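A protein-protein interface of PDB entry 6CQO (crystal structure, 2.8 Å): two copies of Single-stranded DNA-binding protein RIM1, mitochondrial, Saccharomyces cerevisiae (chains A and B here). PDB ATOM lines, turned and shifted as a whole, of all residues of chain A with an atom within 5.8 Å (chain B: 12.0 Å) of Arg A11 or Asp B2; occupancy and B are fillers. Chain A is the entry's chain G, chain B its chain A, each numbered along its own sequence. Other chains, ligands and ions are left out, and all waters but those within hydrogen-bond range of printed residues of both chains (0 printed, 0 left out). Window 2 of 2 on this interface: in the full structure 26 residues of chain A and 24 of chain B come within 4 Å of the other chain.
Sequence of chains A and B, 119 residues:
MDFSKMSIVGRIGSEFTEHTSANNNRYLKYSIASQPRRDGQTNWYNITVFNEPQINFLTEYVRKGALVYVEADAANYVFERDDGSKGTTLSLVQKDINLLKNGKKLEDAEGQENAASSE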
ATOM      1  N   VAL A   9      18.872 -29.279  -0.042  1.00  0.00           N
ATOM      2  CA  VAL A   9      19.576 -28.084   0.405  1.00  0.00           C
ATOM      3  C   VAL A   9      18.664 -26.899   0.131  1.00  0.00           C
ATOM      4  O   VAL A   9      18.285 -26.656  -1.022  1.00  0.00           O
ATOM      5  CB  VAL A   9      20.932 -27.909  -0.295  1.00  0.00           C
ATOM      6  CG1 VAL A   9      21.446 -26.494  -0.096  1.00  0.00           C
ATOM      7  CG2 VAL A   9      21.935 -28.899   0.250  1.00  0.00           C
ATOM      8  N   GLY A  10      18.299 -26.179   1.181  1.00  0.00           N
ATOM      9  CA  GLY A  10      17.391 -25.065   1.019  1.00  0.00           C
ATOM     10  C   GLY A  10      17.348 -24.208   2.262  1.00  0.00           C
ATOM     11  O   GLY A  10      18.086 -24.430   3.222  1.00  0.00           O
ATOM     12  N   ARG A  11      16.460 -23.220   2.228  1.00  0.00           N
ATOM     13  CA  ARG A  11      16.308 -22.251   3.304  1.00  0.00           C
ATOM     14  C   ARG A  11      15.023 -22.537   4.068  1.00  0.00           C
ATOM     15  O   ARG A  11      13.967 -22.741   3.461  1.00  0.00           O
ATOM     16  CB  ARG A  11      16.294 -20.825   2.748  1.00  0.00           C
ATOM     17  CG  ARG A  11      17.624 -20.390   2.146  1.00  0.00           C
ATOM     18  CD  ARG A  11      17.431 -19.483   0.938  1.00  0.00           C
ATOM     19  NE  ARG A  11      16.859 -20.200  -0.201  1.00  0.00           N
ATOM     20  CZ  ARG A  11      15.584 -20.126  -0.570  1.00  0.00           C
ATOM     21  NH1 ARG A  11      14.737 -19.360   0.105  1.00  0.00           N
ATOM     22  NH2 ARG A  11      15.156 -20.815  -1.619  1.00  0.00           N
ATOM     23  N   ILE A  12      15.118 -22.558   5.397  1.00  0.00           N
ATOM     24  CA  ILE A  12      13.956 -22.782   6.249  1.00  0.00           C
ATOM     25  C   ILE A  12      13.049 -21.561   6.178  1.00  0.00           C
ATOM     26  O   ILE A  12      13.329 -20.526   6.792  1.00  0.00           O
ATOM     27  CB  ILE A  12      14.374 -23.080   7.701  1.00  0.00           C
ATOM     28  CG1 ILE A  12      15.228 -24.347   7.761  1.00  0.00           C
ATOM     29  CG2 ILE A  12      13.149 -23.220   8.591  1.00  0.00           C
ATOM     30  CD1 ILE A  12      15.605 -24.763   9.165  1.00  0.00           C
ATOM     31  N   GLY A  13      11.957 -21.672   5.425  1.00  0.00           N
ATOM     32  CA  GLY A  13      11.067 -20.546   5.223  1.00  0.00           C
ATOM     33  C   GLY A  13       9.792 -20.610   6.038  1.00  0.00           C
ATOM     34  O   GLY A  13       8.720 -20.243   5.547  1.00  0.00           O
ATOM     35  N   SER A  31       8.933 -26.039   6.914  1.00  0.00           N
ATOM     36  CA  SER A  31       9.029 -26.080   5.463  1.00  0.00           C
ATOM     37  C   SER A  31      10.399 -25.595   5.011  1.00  0.00           C
ATOM     38  O   SER A  31      11.021 -24.744   5.655  1.00  0.00           O
ATOM     39  CB  SER A  31       7.935 -25.226   4.807  1.00  0.00           C
ATOM     40  OG  SER A  31       6.647 -25.749   5.078  1.00  0.00           O
ATOM     41  N   ILE A  32      10.865 -26.149   3.895  1.00  0.00           N
ATOM     42  CA  ILE A  32      12.147 -25.790   3.301  1.00  0.00           C
ATOM     43  C   ILE A  32      11.886 -25.179   1.932  1.00  0.00           C
ATOM     44  O   ILE A  32      11.172 -25.768   1.111  1.00  0.00           O
ATOM     45  CB  ILE A  32      13.084 -27.005   3.182  1.00  0.00           C
ATOM     46  CG1 ILE A  32      13.447 -27.545   4.566  1.00  0.00           C
ATOM     47  CG2 ILE A  32      14.339 -26.636   2.403  1.00  0.00           C
ATOM     48  CD1 ILE A  32      14.463 -28.665   4.532  1.00  0.00           C
ATOM     49  N   ALA A  33      12.462 -24.004   1.690  1.00  0.00           N
ATOM     50  CA  ALA A  33      12.389 -23.341   0.394  1.00  0.00           C
ATOM     51  C   ALA A  33      13.657 -23.677  -0.382  1.00  0.00           C
ATOM     52  O   ALA A  33      14.743 -23.192  -0.050  1.00  0.00           O
ATOM     53  CB  ALA A  33      12.225 -21.831   0.560  1.00  0.00           C
ATOM     54  N   SER A  34      13.519 -24.511  -1.410  1.00  0.00           N
ATOM     55  CA  SER A  34      14.644 -24.956  -2.228  1.00  0.00           C
ATOM     56  C   SER A  34      14.493 -24.363  -3.623  1.00  0.00           C
ATOM     57  O   SER A  34      13.648 -24.811  -4.407  1.00  0.00           O
ATOM     58  CB  SER A  34      14.711 -26.482  -2.281  1.00  0.00           C
ATOM     59  OG  SER A  34      15.787 -26.920  -3.092  1.00  0.00           O
ATOM     60  N   GLN A  35      15.311 -23.357  -3.931  1.00  0.00           N
ATOM     61  CA  GLN A  35      15.289 -22.705  -5.236  1.00  0.00           C
ATOM     62  C   GLN A  35      16.591 -23.007  -5.970  1.00  0.00           C
ATOM     63  O   GLN A  35      17.602 -22.327  -5.745  1.00  0.00           O
ATOM     64  CB  GLN A  35      15.098 -21.192  -5.084  1.00  0.00           C
ATOM     65  CG  GLN A  35      14.590 -20.503  -6.340  1.00  0.00           C
ATOM     66  CD  GLN A  35      14.452 -19.000  -6.175  1.00  0.00           C
ATOM     67  OE1 GLN A  35      15.273 -18.356  -5.522  1.00  0.00           O
ATOM     68  NE2 GLN A  35      13.407 -18.435  -6.770  1.00  0.00           N
ATOM     69  N   PRO A  36      16.620 -24.017  -6.846  1.00  0.00           N
ATOM     70  CA  PRO A  36      17.882 -24.350  -7.526  1.00  0.00           C
ATOM     71  C   PRO A  36      18.359 -23.271  -8.483  1.00  0.00           C
ATOM     72  O   PRO A  36      19.565 -23.189  -8.746  1.00  0.00           O
ATOM     73  CB  PRO A  36      17.548 -25.652  -8.269  1.00  0.00           C
ATOM     74  CG  PRO A  36      16.314 -26.184  -7.599  1.00  0.00           C
ATOM     75  CD  PRO A  36      15.551 -24.975  -7.161  1.00  0.00           C
ATOM     76  N   ARG A  37      17.457 -22.447  -9.010  1.00  0.00           N
ATOM     77  CA  ARG A  37      17.798 -21.423  -9.987  1.00  0.00           C
ATOM     78  C   ARG A  37      17.368 -20.056  -9.479  1.00  0.00           C
ATOM     79  O   ARG A  37      16.279 -19.905  -8.914  1.00  0.00           O
ATOM     80  CB  ARG A  37      17.135 -21.704 -11.337  1.00  0.00           C
ATOM     81  CG  ARG A  37      17.419 -23.091 -11.886  1.00  0.00           C
ATOM     82  CD  ARG A  37      18.747 -23.150 -12.630  1.00  0.00           C
ATOM     83  NE  ARG A  37      19.532 -24.335 -12.287  1.00  0.00           N
ATOM     84  CZ  ARG A  37      19.237 -25.571 -12.677  1.00  0.00           C
ATOM     85  NH1 ARG A  37      18.161 -25.798 -13.417  1.00  0.00           N
ATOM     86  NH2 ARG A  37      20.013 -26.585 -12.318  1.00  0.00           N
ATOM     87  N   THR A  42      10.717 -22.100  -7.045  1.00  0.00           N
ATOM     88  CA  THR A  42      11.077 -22.466  -5.681  1.00  0.00           C
ATOM     89  C   THR A  42      10.307 -23.717  -5.276  1.00  0.00           C
ATOM     90  O   THR A  42       9.083 -23.780  -5.440  1.00  0.00           O
ATOM     91  CB  THR A  42      10.778 -21.323  -4.708  1.00  0.00           C
ATOM     92  OG1 THR A  42      11.569 -20.179  -5.054  1.00  0.00           O
ATOM     93  CG2 THR A  42      11.098 -21.736  -3.277  1.00  0.00           C
ATOM     94  N   TRP A  44       9.000 -26.225  -2.328  1.00  0.00           N
ATOM     95  CA  TRP A  44       8.642 -26.219  -0.916  1.00  0.00           C
ATOM     96  C   TRP A  44       8.413 -27.647  -0.444  1.00  0.00           C
ATOM     97  O   TRP A  44       7.625 -28.386  -1.046  1.00  0.00           O
ATOM     98  CB  TRP A  44       7.393 -25.374  -0.668  1.00  0.00           C
ATOM     99  CG  TRP A  44       7.643 -23.906  -0.764  1.00  0.00           C
ATOM    100  CD1 TRP A  44       7.590 -23.137  -1.889  1.00  0.00           C
ATOM    101  CD2 TRP A  44       7.992 -23.023   0.309  1.00  0.00           C
ATOM    102  NE1 TRP A  44       7.882 -21.830  -1.584  1.00  0.00           N
ATOM    103  CE2 TRP A  44       8.132 -21.733  -0.241  1.00  0.00           C
ATOM    104  CE3 TRP A  44       8.197 -23.198   1.682  1.00  0.00           C
ATOM    105  CZ2 TRP A  44       8.468 -20.625   0.534  1.00  0.00           C
ATOM    106  CZ3 TRP A  44       8.531 -22.096   2.448  1.00  0.00           C
ATOM    107  CH2 TRP A  44       8.663 -20.826   1.873  1.00  0.00           C
ATOM    108  N   GLY A  65      14.916 -18.874   7.827  1.00  0.00           N
ATOM    109  CA  GLY A  65      15.763 -18.427   6.742  1.00  0.00           C
ATOM    110  C   GLY A  65      17.144 -19.042   6.710  1.00  0.00           C
ATOM    111  O   GLY A  65      17.958 -18.650   5.865  1.00  0.00           O
ATOM    112  N   ALA A  66      17.438 -19.991   7.598  1.00  0.00           N
ATOM    113  CA  ALA A  66      18.753 -20.611   7.627  1.00  0.00           C
ATOM    114  C   ALA A  66      18.909 -21.600   6.478  1.00  0.00           C
ATOM    115  O   ALA A  66      17.967 -22.307   6.109  1.00  0.00           O
ATOM    116  CB  ALA A  66      18.978 -21.318   8.962  1.00  0.00           C
ATOM    117  N   LEU A  67      20.112 -21.644   5.911  1.00  0.00           N
ATOM    118  CA  LEU A  67      20.424 -22.600   4.856  1.00  0.00           C
ATOM    119  C   LEU A  67      20.847 -23.921   5.487  1.00  0.00           C
ATOM    120  O   LEU A  67      21.843 -23.975   6.215  1.00  0.00           O
ATOM    121  CB  LEU A  67      21.525 -22.056   3.951  1.00  0.00           C
ATOM    122  CG  LEU A  67      21.982 -22.974   2.819  1.00  0.00           C
ATOM    123  CD1 LEU A  67      20.841 -23.256   1.853  1.00  0.00           C
ATOM    124  CD2 LEU A  67      23.171 -22.367   2.090  1.00  0.00           C
ATOM    125  N   VAL A  68      20.095 -24.985   5.206  1.00  0.00           N
ATOM    126  CA  VAL A  68      20.338 -26.286   5.809  1.00  0.00           C
ATOM    127  C   VAL A  68      20.411 -27.344   4.718  1.00  0.00           C
ATOM    128  O   VAL A  68      19.878 -27.181   3.618  1.00  0.00           O
ATOM    129  CB  VAL A  68      19.254 -26.665   6.841  1.00  0.00           C
ATOM    130  CG1 VAL A  68      19.235 -25.671   7.989  1.00  0.00           C
ATOM    131  CG2 VAL A  68      17.886 -26.743   6.172  1.00  0.00           C
ATOM    132  N   MET B   1      23.323 -24.374  -6.355  1.00  0.00           N
ATOM    133  CA  MET B   1      23.318 -24.121  -4.918  1.00  0.00           C
ATOM    134  C   MET B   1      22.305 -25.011  -4.206  1.00  0.00           C
ATOM    135  O   MET B   1      22.668 -26.003  -3.574  1.00  0.00           O
ATOM    136  CB  MET B   1      23.014 -22.649  -4.635  1.00  0.00           C
ATOM    137  CG  MET B   1      24.069 -21.935  -3.800  1.00  0.00           C
ATOM    138  SD  MET B   1      24.526 -22.882  -2.156  1.00  0.00           S
ATOM    139  CE  MET B   1      26.171 -23.750  -2.746  1.00  0.00           C
ATOM    140  N   ASP B   2      21.031 -24.643  -4.308  1.00  0.00           N
ATOM    141  CA  ASP B   2      19.960 -25.449  -3.744  1.00  0.00           C
ATOM    142  C   ASP B   2      19.600 -26.586  -4.691  1.00  0.00           C
ATOM    143  O   ASP B   2      19.751 -26.478  -5.912  1.00  0.00           O
ATOM    144  CB  ASP B   2      18.726 -24.587  -3.474  1.00  0.00           C
ATOM    145  CG  ASP B   2      18.979 -23.513  -2.434  1.00  0.00           C
ATOM    146  OD1 ASP B   2      20.145 -23.349  -2.016  1.00  0.00           O
ATOM    147  OD2 ASP B   2      18.012 -22.827  -2.039  1.00  0.00           O
ATOM    148  N   PHE B   3      19.123 -27.688  -4.117  1.00  0.00           N
ATOM    149  CA  PHE B   3      18.694 -28.826  -4.918  1.00  0.00           C
ATOM    150  C   PHE B   3      17.847 -29.751  -4.058  1.00  0.00           C
ATOM    151  O   PHE B   3      17.839 -29.657  -2.828  1.00  0.00           O
ATOM    152  CB  PHE B   3      19.886 -29.591  -5.507  1.00  0.00           C
ATOM    153  CG  PHE B   3      20.653 -30.395  -4.497  1.00  0.00           C
ATOM    154  CD1 PHE B   3      21.641 -29.805  -3.730  1.00  0.00           C
ATOM    155  CD2 PHE B   3      20.391 -31.745  -4.319  1.00  0.00           C
ATOM    156  CE1 PHE B   3      22.350 -30.540  -2.802  1.00  0.00           C
ATOM    157  CE2 PHE B   3      21.096 -32.485  -3.390  1.00  0.00           C
ATOM    158  CZ  PHE B   3      22.077 -31.883  -2.631  1.00  0.00           C
ATOM    159  N   SER B   4      17.138 -30.652  -4.733  1.00  0.00           N
ATOM    160  CA  SER B   4      16.353 -31.693  -4.076  1.00  0.00           C
ATOM    161  C   SER B   4      16.411 -32.931  -4.958  1.00  0.00           C
ATOM    162  O   SER B   4      15.774 -32.974  -6.015  1.00  0.00           O
ATOM    163  CB  SER B   4      14.909 -31.246  -3.843  1.00  0.00           C
ATOM    164  OG  SER B   4      14.281 -30.888  -5.061  1.00  0.00           O
ATOM    165  N   LYS B   5      17.182 -33.927  -4.532  1.00  0.00           N
ATOM    166  CA  LYS B   5      17.386 -35.149  -5.289  1.00  0.00           C
ATOM    167  C   LYS B   5      16.894 -36.338  -4.476  1.00  0.00           C
ATOM    168  O   LYS B   5      16.871 -36.298  -3.242  1.00  0.00           O
ATOM    169  CB  LYS B   5      18.868 -35.323  -5.651  1.00  0.00           C
ATOM    170  CG  LYS B   5      19.129 -36.212  -6.851  1.00  0.00           C
ATOM    171  CD  LYS B   5      20.583 -36.127  -7.286  1.00  0.00           C
ATOM    172  CE  LYS B   5      20.819 -36.898  -8.574  1.00  0.00           C
ATOM    173  NZ  LYS B   5      22.223 -36.769  -9.047  1.00  0.00           N
ATOM    174  N   MET B   6      16.493 -37.396  -5.173  1.00  0.00           N
ATOM    175  CA  MET B   6      15.984 -38.585  -4.500  1.00  0.00           C
ATOM    176  C   MET B   6      16.497 -39.882  -5.121  1.00  0.00           C
ATOM    177  O   MET B   6      16.497 -40.043  -6.342  1.00  0.00           O
ATOM    178  CB  MET B   6      14.454 -38.586  -4.502  1.00  0.00           C
ATOM    179  CG  MET B   6      13.843 -39.827  -3.866  1.00  0.00           C
ATOM    180  SD  MET B   6      11.909 -39.735  -3.669  1.00  0.00           S
ATOM    181  CE  MET B   6      11.795 -38.096  -2.637  1.00  0.00           C
ATOM    182  N   ALA B  72      16.816 -39.431  -9.073  1.00  0.00           N
ATOM    183  CA  ALA B  72      15.955 -38.462  -9.735  1.00  0.00           C
ATOM    184  C   ALA B  72      16.019 -37.117  -9.030  1.00  0.00           C
ATOM    185  O   ALA B  72      16.129 -37.053  -7.804  1.00  0.00           O
ATOM    186  CB  ALA B  72      14.502 -38.954  -9.780  1.00  0.00           C
ATOM    187  N   ASP B  73      15.947 -36.045  -9.816  1.00  0.00           N
ATOM    188  CA  ASP B  73      15.828 -34.701  -9.267  1.00  0.00           C
ATOM    189  C   ASP B  73      14.372 -34.424  -8.915  1.00  0.00           C
ATOM    190  O   ASP B  73      13.477 -34.604  -9.747  1.00  0.00           O
ATOM    191  CB  ASP B  73      16.345 -33.662 -10.261  1.00  0.00           C
ATOM    192  CG  ASP B  73      17.858 -33.654 -10.366  1.00  0.00           C
ATOM    193  OD1 ASP B  73      18.528 -34.018  -9.376  1.00  0.00           O
ATOM    194  OD2 ASP B  73      18.379 -33.277 -11.436  1.00  0.00           O
ATOM    195  N   ALA B  74      14.137 -33.983  -7.683  1.00  0.00           N
ATOM    196  CA  ALA B  74      12.792 -33.793  -7.164  1.00  0.00           C
ATOM    197  C   ALA B  74      12.385 -32.328  -7.249  1.00  0.00           C
ATOM    198  O   ALA B  74      13.177 -31.431  -6.944  1.00  0.00           O
ATOM    199  CB  ALA B  74      12.697 -34.278  -5.717  1.00  0.00           C
ATOM    200  N   ALA B  75      11.140 -32.099  -7.663  1.00  0.00           N
ATOM    201  CA  ALA B  75      10.549 -30.770  -7.713  1.00  0.00           C
ATOM    202  C   ALA B  75       9.144 -30.839  -7.138  1.00  0.00           C
ATOM    203  O   ALA B  75       8.430 -31.825  -7.343  1.00  0.00           O
ATOM    204  CB  ALA B  75      10.509 -30.226  -9.146  1.00  0.00           C
ATOM    205  N   ASN B  76       8.748 -29.793  -6.415  1.00  0.00           N
ATOM    206  CA  ASN B  76       7.447 -29.737  -5.752  1.00  0.00           C
ATOM    207  C   ASN B  76       6.698 -28.516  -6.280  1.00  0.00           C
ATOM    208  O   ASN B  76       6.988 -27.383  -5.886  1.00  0.00           O
ATOM    209  CB  ASN B  76       7.611 -29.685  -4.236  1.00  0.00           C
ATOM    210  CG  ASN B  76       6.710 -30.669  -3.517  1.00  0.00           C
ATOM    211  OD1 ASN B  76       6.177 -31.598  -4.124  1.00  0.00           O
ATOM    212  ND2 ASN B  76       6.541 -30.476  -2.215  1.00  0.00           N
ATOM    213  N   LYS B  95      17.474 -39.226 -13.631  1.00  0.00           N
ATOM    214  CA  LYS B  95      18.821 -38.886 -14.068  1.00  0.00           C
ATOM    215  C   LYS B  95      19.712 -40.095 -14.297  1.00  0.00           C
ATOM    216  O   LYS B  95      20.634 -40.015 -15.111  1.00  0.00           O
ATOM    217  CB  LYS B  95      19.496 -37.953 -13.051  1.00  0.00           C
ATOM    218  CG  LYS B  95      18.887 -36.563 -12.999  1.00  0.00           C
ATOM    219  CD  LYS B  95      18.917 -35.906 -14.371  1.00  0.00           C
ATOM    220  CE  LYS B  95      18.163 -34.588 -14.373  1.00  0.00           C
ATOM    221  NZ  LYS B  95      18.156 -33.955 -15.721  1.00  0.00           N
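Hydrophobic or aromatic side chains of chain A that line the printed part of chain B: Val A9, Pro A36 and Leu A67.
Along chain A the printed residues that touch a printed residue of chain B span positions 9 to 67.
Printed residues of chain B that touch a printed residue of chain A: Met B1, Asp B2, Phe B3 and Asn B76.
Hydrophobic or aromatic side chains of chain B that line the printed part of chain A: Phe B3.
Among the printed residues, 12 pairs touch across the chains.
Among the printed residues, Asp or Glu carboxylates within 4 Å of a Lys or Arg side-chain nitrogen of the other chain: Arg A11 with Asp B2.
The side-chain carboxylate of Asp B2 is in salt-bridge range of the guanidinium group of Arg A11 (3.4 Å).
OD2 of Asp B2 is in hydrogen-bond range of N of Gln A35, at 3.3 Å.
The backbone carbonyl oxygen (O) of Phe B3 sits at hydrogen-bond distance from the backbone NH (N) of Val A9 (3.0 Å).
The side-chain hydroxyl (OG) of Ser A34 lies within hydrogen-bond range of the backbone carbonyl oxygen (O) of Phe B3 (3.4 Å).
The backbone carbonyl oxygen (O) of Trp A44 sits at hydrogen-bond distance from the side-chain amide nitrogen (ND2) of Asn B76 (2.6 Å).
O of Val A9 lies within hydrogen-bond range of OG of Ser A34 (3.3 Å).
The backbone NH (N) of Val A68 is in hydrogen-bond range of the backbone carbonyl oxygen (O) of Gly A10, at 2.9 Å.
N of Ala A33 is in hydrogen-bond range of O of Arg A11 (2.6 Å).
The side-chain amide nitrogen (NE2) of Gln A35 lies within hydrogen-bond range of the side-chain hydroxyl (OG1) of Thr A42 (3.1 Å).
Gly A10 touches one residue of chain B.
No residue of chain B comes within 4 Å of Ile A12.
Ser A31 touches none of the printed residues of chain B.
Ala A33 touches just one residue of chain B: Asp B2.
Pro A36 touches just one residue of chain B: Asp B2.
No residue of chain B comes within 4 Å of Arg A37.
No residue of chain B comes within 4 Å of Thr A42.
Of the printed residues of chain B, Trp A44 touches Asn B76.
Printed residues of chain B within 4 Å of Leu A67: Asp B2 (3.9 Å).
No residue of chain B comes within 4 Å of Val A68.
Printed residues of chain A within 4 Å of Met B1: Val A9.
Asp B2 touches just these residues of chain A: Val A9, Gly A10, Arg A11, Ala A33, Ser A34, Gln A35, Pro A36 and Leu A67.
Printed residues of chain A within 4 Å of Phe B3: Val A9 and Ser A34.
Of the printed residues of chain A, Asn B76 touches Trp A44 (2.6 Å).
The nearest residue of chain A that does not touch Asp B2 is Arg A37 (5.6 Å).
No position is printed for both chains.
Among the printed residues, pairs that only touch across the chains: Val A9 with Met B1, Val A9 with Asp B2, Gly A10 with Asp B2, Ala A33 with Asp B2, Ser A34 with Asp B2, Pro A36 with Asp B2 and Leu A67 with Asp B2.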
